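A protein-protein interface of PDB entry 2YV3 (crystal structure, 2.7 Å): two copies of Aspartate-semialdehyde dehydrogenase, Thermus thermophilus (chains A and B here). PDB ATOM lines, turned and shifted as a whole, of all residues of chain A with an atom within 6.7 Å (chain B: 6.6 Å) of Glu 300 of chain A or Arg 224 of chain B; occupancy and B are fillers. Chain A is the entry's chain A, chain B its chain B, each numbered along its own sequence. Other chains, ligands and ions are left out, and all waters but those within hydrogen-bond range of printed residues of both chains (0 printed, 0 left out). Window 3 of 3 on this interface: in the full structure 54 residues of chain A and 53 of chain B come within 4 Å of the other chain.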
ATOM      1  N   GLU A 245      23.986  -0.150  25.409  1.00  0.00           N
ATOM      2  CA  GLU A 245      25.099  -0.652  24.627  1.00  0.00           C
ATOM      3  C   GLU A 245      25.595  -1.814  25.492  1.00  0.00           C
ATOM      4  O   GLU A 245      25.780  -1.654  26.703  1.00  0.00           O
ATOM      5  CB  GLU A 245      26.178   0.425  24.452  1.00  0.00           C
ATOM      6  CG  GLU A 245      27.324   0.010  23.527  1.00  0.00           C
ATOM      7  CD  GLU A 245      28.328   1.128  23.294  1.00  0.00           C
ATOM      8  OE1 GLU A 245      28.822   1.715  24.291  1.00  0.00           O
ATOM      9  OE2 GLU A 245      28.633   1.409  22.112  1.00  0.00           O
ATOM     10  N   SER A 296      19.219  -2.146  18.273  1.00  0.00           N
ATOM     11  CA  SER A 296      19.563  -0.733  18.211  1.00  0.00           C
ATOM     12  C   SER A 296      20.448  -0.347  17.027  1.00  0.00           C
ATOM     13  O   SER A 296      21.423  -1.041  16.715  1.00  0.00           O
ATOM     14  CB  SER A 296      20.278  -0.315  19.494  1.00  0.00           C
ATOM     15  OG  SER A 296      20.905   0.946  19.318  1.00  0.00           O
ATOM     16  N   LEU A 297      20.126   0.762  16.375  1.00  0.00           N
ATOM     17  CA  LEU A 297      20.963   1.211  15.279  1.00  0.00           C
ATOM     18  C   LEU A 297      22.006   2.215  15.783  1.00  0.00           C
ATOM     19  O   LEU A 297      23.072   2.374  15.187  1.00  0.00           O
ATOM     20  CB  LEU A 297      20.110   1.809  14.159  1.00  0.00           C
ATOM     21  CG  LEU A 297      19.509   0.740  13.225  1.00  0.00           C
ATOM     22  CD1 LEU A 297      20.608  -0.032  12.515  1.00  0.00           C
ATOM     23  CD2 LEU A 297      18.678  -0.221  14.021  1.00  0.00           C
ATOM     24  N   ALA A 298      21.707   2.867  16.902  1.00  0.00           N
ATOM     25  CA  ALA A 298      22.621   3.848  17.488  1.00  0.00           C
ATOM     26  C   ALA A 298      23.949   3.195  17.855  1.00  0.00           C
ATOM     27  O   ALA A 298      24.996   3.579  17.351  1.00  0.00           O
ATOM     28  CB  ALA A 298      21.992   4.485  18.728  1.00  0.00           C
ATOM     29  N   PHE A 299      23.893   2.198  18.731  1.00  0.00           N
ATOM     30  CA  PHE A 299      25.087   1.480  19.175  1.00  0.00           C
ATOM     31  C   PHE A 299      25.444   0.316  18.249  1.00  0.00           C
ATOM     32  O   PHE A 299      24.586  -0.217  17.534  1.00  0.00           O
ATOM     33  CB  PHE A 299      24.852   0.952  20.575  1.00  0.00           C
ATOM     34  CG  PHE A 299      24.467   2.013  21.549  1.00  0.00           C
ATOM     35  CD1 PHE A 299      23.479   1.776  22.509  1.00  0.00           C
ATOM     36  CD2 PHE A 299      25.100   3.255  21.520  1.00  0.00           C
ATOM     37  CE1 PHE A 299      23.128   2.758  23.428  1.00  0.00           C
ATOM     38  CE2 PHE A 299      24.757   4.239  22.426  1.00  0.00           C
ATOM     39  CZ  PHE A 299      23.763   3.988  23.388  1.00  0.00           C
ATOM     40  N   GLU A 300      26.713  -0.077  18.275  1.00  0.00           N
ATOM     41  CA  GLU A 300      27.172  -1.177  17.433  1.00  0.00           C
ATOM     42  C   GLU A 300      26.761  -2.530  18.033  1.00  0.00           C
ATOM     43  O   GLU A 300      26.876  -3.561  17.394  1.00  0.00           O
ATOM     44  CB  GLU A 300      28.685  -1.094  17.234  1.00  0.00           C
ATOM     45  CG  GLU A 300      29.122  -1.233  15.775  1.00  0.00           C
ATOM     46  CD  GLU A 300      28.895  -2.637  15.229  1.00  0.00           C
ATOM     47  OE1 GLU A 300      28.763  -3.565  16.058  1.00  0.00           O
ATOM     48  OE2 GLU A 300      28.865  -2.817  13.985  1.00  0.00           O
ATOM     49  N   ASN A 301      26.299  -2.512  19.274  1.00  0.00           N
ATOM     50  CA  ASN A 301      25.795  -3.711  19.930  1.00  0.00           C
ATOM     51  C   ASN A 301      24.783  -3.209  20.958  1.00  0.00           C
ATOM     52  O   ASN A 301      25.020  -3.218  22.158  1.00  0.00           O
ATOM     53  CB  ASN A 301      26.918  -4.499  20.607  1.00  0.00           C
ATOM     54  CG  ASN A 301      26.437  -5.840  21.151  1.00  0.00           C
ATOM     55  OD1 ASN A 301      25.517  -6.445  20.614  1.00  0.00           O
ATOM     56  ND2 ASN A 301      27.075  -6.308  22.205  1.00  0.00           N
ATOM     57  N   GLY A 302      23.649  -2.748  20.455  1.00  0.00           N
ATOM     58  CA  GLY A 302      22.645  -2.198  21.329  1.00  0.00           C
ATOM     59  C   GLY A 302      21.238  -2.693  21.111  1.00  0.00           C
ATOM     60  O   GLY A 302      20.952  -3.507  20.219  1.00  0.00           O
ATOM     61  N   LYS B 144      27.612  12.223  15.333  1.00  0.00           N
ATOM     62  CA  LYS B 144      28.092  10.871  15.070  1.00  0.00           C
ATOM     63  C   LYS B 144      27.113   9.824  15.560  1.00  0.00           C
ATOM     64  O   LYS B 144      27.087   8.701  15.061  1.00  0.00           O
ATOM     65  CB  LYS B 144      29.434  10.624  15.765  1.00  0.00           C
ATOM     66  CG  LYS B 144      30.662  11.205  15.074  1.00  0.00           C
ATOM     67  CD  LYS B 144      31.933  10.798  15.820  1.00  0.00           C
ATOM     68  CE  LYS B 144      32.111   9.272  15.852  1.00  0.00           C
ATOM     69  NZ  LYS B 144      33.118   8.841  16.858  1.00  0.00           N
ATOM     70  N   ARG B 145      26.321  10.199  16.555  1.00  0.00           N
ATOM     71  CA  ARG B 145      25.351   9.299  17.158  1.00  0.00           C
ATOM     72  C   ARG B 145      24.245  10.097  17.792  1.00  0.00           C
ATOM     73  O   ARG B 145      24.479  10.807  18.753  1.00  0.00           O
ATOM     74  CB  ARG B 145      26.025   8.470  18.232  1.00  0.00           C
ATOM     75  CG  ARG B 145      26.982   7.468  17.675  1.00  0.00           C
ATOM     76  CD  ARG B 145      26.353   6.098  17.732  1.00  0.00           C
ATOM     77  NE  ARG B 145      26.365   5.610  19.095  1.00  0.00           N
ATOM     78  CZ  ARG B 145      27.475   5.293  19.738  1.00  0.00           C
ATOM     79  NH1 ARG B 145      28.637   5.415  19.117  1.00  0.00           N
ATOM     80  NH2 ARG B 145      27.423   4.876  20.999  1.00  0.00           N
ATOM     81  N   VAL B 146      23.046   9.984  17.239  1.00  0.00           N
ATOM     82  CA  VAL B 146      21.888  10.681  17.762  1.00  0.00           C
ATOM     83  C   VAL B 146      20.929   9.622  18.281  1.00  0.00           C
ATOM     84  O   VAL B 146      20.846   8.521  17.731  1.00  0.00           O
ATOM     85  CB  VAL B 146      21.183  11.507  16.656  1.00  0.00           C
ATOM     86  CG1 VAL B 146      19.776  11.910  17.083  1.00  0.00           C
ATOM     87  CG2 VAL B 146      21.999  12.736  16.339  1.00  0.00           C
ATOM     88  N   ILE B 147      20.237   9.946  19.363  1.00  0.00           N
ATOM     89  CA  ILE B 147      19.250   9.066  19.962  1.00  0.00           C
ATOM     90  C   ILE B 147      18.146  10.023  20.376  1.00  0.00           C
ATOM     91  O   ILE B 147      18.395  10.969  21.150  1.00  0.00           O
ATOM     92  CB  ILE B 147      19.800   8.364  21.202  1.00  0.00           C
ATOM     93  CG1 ILE B 147      20.936   7.426  20.790  1.00  0.00           C
ATOM     94  CG2 ILE B 147      18.677   7.611  21.918  1.00  0.00           C
ATOM     95  CD1 ILE B 147      21.666   6.766  21.946  1.00  0.00           C
ATOM     96  N   VAL B 211      15.563   9.190  10.468  1.00  0.00           N
ATOM     97  CA  VAL B 211      16.920   8.785  10.100  1.00  0.00           C
ATOM     98  C   VAL B 211      17.130   9.056   8.603  1.00  0.00           C
ATOM     99  O   VAL B 211      17.795  10.030   8.224  1.00  0.00           O
ATOM    100  CB  VAL B 211      17.143   7.274  10.341  1.00  0.00           C
ATOM    101  CG1 VAL B 211      18.567   6.880   9.936  1.00  0.00           C
ATOM    102  CG2 VAL B 211      16.851   6.929  11.783  1.00  0.00           C
ATOM    103  N   HIS B 215      19.700  11.709   6.883  1.00  0.00           N
ATOM    104  CA  HIS B 215      20.852  11.431   6.034  1.00  0.00           C
ATOM    105  C   HIS B 215      20.855  12.273   4.750  1.00  0.00           C
ATOM    106  O   HIS B 215      21.876  12.873   4.405  1.00  0.00           O
ATOM    107  CB  HIS B 215      20.901   9.950   5.645  1.00  0.00           C
ATOM    108  CG  HIS B 215      21.270   9.036   6.773  1.00  0.00           C
ATOM    109  ND1 HIS B 215      21.379   7.671   6.615  1.00  0.00           N
ATOM    110  CD2 HIS B 215      21.552   9.287   8.075  1.00  0.00           C
ATOM    111  CE1 HIS B 215      21.712   7.119   7.768  1.00  0.00           C
ATOM    112  NE2 HIS B 215      21.823   8.079   8.670  1.00  0.00           N
ATOM    113  N   ASP B 221      25.816  10.315   4.930  1.00  0.00           N
ATOM    114  CA  ASP B 221      25.291   8.944   4.958  1.00  0.00           C
ATOM    115  C   ASP B 221      25.728   8.292   6.264  1.00  0.00           C
ATOM    116  O   ASP B 221      25.012   7.466   6.813  1.00  0.00           O
ATOM    117  CB  ASP B 221      25.834   8.135   3.759  1.00  0.00           C
ATOM    118  CG  ASP B 221      24.806   7.128   3.182  1.00  0.00           C
ATOM    119  OD1 ASP B 221      24.355   6.225   3.921  1.00  0.00           O
ATOM    120  OD2 ASP B 221      24.452   7.233   1.979  1.00  0.00           O
ATOM    121  N   THR B 222      26.889   8.711   6.766  1.00  0.00           N
ATOM    122  CA  THR B 222      27.493   8.179   7.991  1.00  0.00           C
ATOM    123  C   THR B 222      27.167   8.894   9.294  1.00  0.00           C
ATOM    124  O   THR B 222      27.873   9.820   9.662  1.00  0.00           O
ATOM    125  CB  THR B 222      29.034   8.184   7.873  1.00  0.00           C
ATOM    126  OG1 THR B 222      29.622   7.996   9.166  1.00  0.00           O
ATOM    127  CG2 THR B 222      29.519   9.514   7.312  1.00  0.00           C
ATOM    128  N   ILE B 223      26.131   8.456  10.007  1.00  0.00           N
ATOM    129  CA  ILE B 223      25.744   9.072  11.295  1.00  0.00           C
ATOM    130  C   ILE B 223      24.780   8.155  12.065  1.00  0.00           C
ATOM    131  O   ILE B 223      23.567   8.317  11.978  1.00  0.00           O
ATOM    132  CB  ILE B 223      25.064  10.466  11.082  1.00  0.00           C
ATOM    133  CG1 ILE B 223      26.085  11.470  10.549  1.00  0.00           C
ATOM    134  CG2 ILE B 223      24.461  10.981  12.398  1.00  0.00           C
ATOM    135  CD1 ILE B 223      25.618  12.914  10.538  1.00  0.00           C
ATOM    136  N   ARG B 224      25.326   7.200  12.812  1.00  0.00           N
ATOM    137  CA  ARG B 224      24.521   6.229  13.568  1.00  0.00           C
ATOM    138  C   ARG B 224      23.329   6.876  14.271  1.00  0.00           C
ATOM    139  O   ARG B 224      23.435   7.276  15.423  1.00  0.00           O
ATOM    140  CB  ARG B 224      25.382   5.507  14.620  1.00  0.00           C
ATOM    141  CG  ARG B 224      26.857   5.342  14.256  1.00  0.00           C
ATOM    142  CD  ARG B 224      27.143   4.117  13.397  1.00  0.00           C
ATOM    143  NE  ARG B 224      27.356   2.917  14.201  1.00  0.00           N
ATOM    144  CZ  ARG B 224      26.579   1.840  14.158  1.00  0.00           C
ATOM    145  NH1 ARG B 224      26.850   0.791  14.925  1.00  0.00           N
ATOM    146  NH2 ARG B 224      25.529   1.810  13.347  1.00  0.00           N
ATOM    147  N   ILE B 225      22.193   6.975  13.586  1.00  0.00           N
ATOM    148  CA  ILE B 225      21.012   7.585  14.184  1.00  0.00           C
ATOM    149  C   ILE B 225      20.097   6.514  14.801  1.00  0.00           C
ATOM    150  O   ILE B 225      20.250   5.319  14.522  1.00  0.00           O
ATOM    151  CB  ILE B 225      20.267   8.481  13.141  1.00  0.00           C
ATOM    152  CG1 ILE B 225      20.970   9.840  13.052  1.00  0.00           C
ATOM    153  CG2 ILE B 225      18.834   8.731  13.557  1.00  0.00           C
ATOM    154  CD1 ILE B 225      20.579  10.683  11.865  1.00  0.00           C
ATOM    155  N   SER B 226      19.168   6.942  15.657  1.00  0.00           N
ATOM    156  CA  SER B 226      18.274   6.016  16.337  1.00  0.00           C
ATOM    157  C   SER B 226      17.073   6.756  16.930  1.00  0.00           C
ATOM    158  O   SER B 226      17.229   7.578  17.839  1.00  0.00           O
ATOM    159  CB  SER B 226      19.055   5.310  17.454  1.00  0.00           C
ATOM    160  OG  SER B 226      18.605   3.989  17.665  1.00  0.00           O
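N of Glu 300 of chain A lies close to NH1 of Arg 224 of chain B (3.5 Å).
OG of Ser 226 of chain B sits at hydrogen-bond distance from N of Ala 298 of chain A.
NH2 of Arg 145 of chain B lies within salt-bridge range of OE2 of Glu 245 of chain A, 3.8 Å away.
NH2 of Arg 224 of chain B sits at hydrogen-bond distance from O of Leu 297 of chain A.
O of Ala 298 of chain A lies close to NE of Arg 145 of chain B (3.0 Å).
The side-chain hydroxyl (OG) of Ser 296 of chain A sits at hydrogen-bond distance from the backbone NH (N) of Phe 299 of chain A (3.3 Å).
O of Arg 224 of chain B sits at hydrogen-bond distance from N of Val 146 of chain B, 3.3 Å away.
O of Lys 144 of chain B lies within hydrogen-bond range of N of Arg 224 of chain B, at 3.2 Å.
The backbone NH (N) of Ser 226 of chain B lies within hydrogen-bond range of the backbone carbonyl oxygen (O) of Val 146 of chain B.
The backbone NH of Ala 298 of chain A sits at hydrogen-bond distance from the side-chain hydroxyl of Ser 296 of chain A, 3.2 Å away.
Ile 225 of chain B touches Leu 297 of chain A.
Leu 297 of chain A touches Ser 226 of chain B (N to OG, 3.8 Å).
CG1 of Ile 147 of chain B touches CB of Ala 298 of chain A, 3.7 Å away.
Ala 298 of chain A touches Arg 224 of chain B (O to CB, 3.4 Å).
Ala 298 of chain A touches Ile 225 of chain B (N to O, 3.7 Å).
Arg 145 of chain B touches Phe 299 of chain A (NH2 to CD2, 2.9 Å).
Phe 299 of chain A touches Ile 147 of chain B (CZ to CD1, 3.8 Å).
Phe 299 of chain A touches Arg 224 of chain B (O to NH1, 3.6 Å).
Of the printed residues of chain B, Glu 245 of chain A touches Arg 145 (3.8 Å).
Of chain B, only Arg 224 (3.2 Å) comes within 4 Å of Glu 300 of chain A.
Lys 144 of chain B touches none of the printed residues of chain A.
Of the printed residues of chain A, Arg 145 of chain B touches Glu 245, Ala 298 and Phe 299.
Of the printed residues of chain A, Ser 226 of chain B touches Leu 297 (3.8 Å) and Ala 298 (3.3 Å).
The nearest residue of chain A that does not touch Arg 224 of chain B is Asn 301 of chain A (5.5 Å).
Of the 8 printed residues of chain A, 5 touch a printed residue of chain B.
Printed residues of chain B that touch a printed residue of chain A: Arg 145, Ile 147, Arg 224, Ile 225 and Ser 226.
Along chain B the printed residues that touch a printed residue of chain A span positions 145 to 226.
Among the printed residues, Asp or Glu carboxylates within 4 Å of a Lys or Arg side-chain nitrogen of the other chain: Glu 245 of chain A with Arg 145 of chain B (3.8 Å).
No position is printed for both chains.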
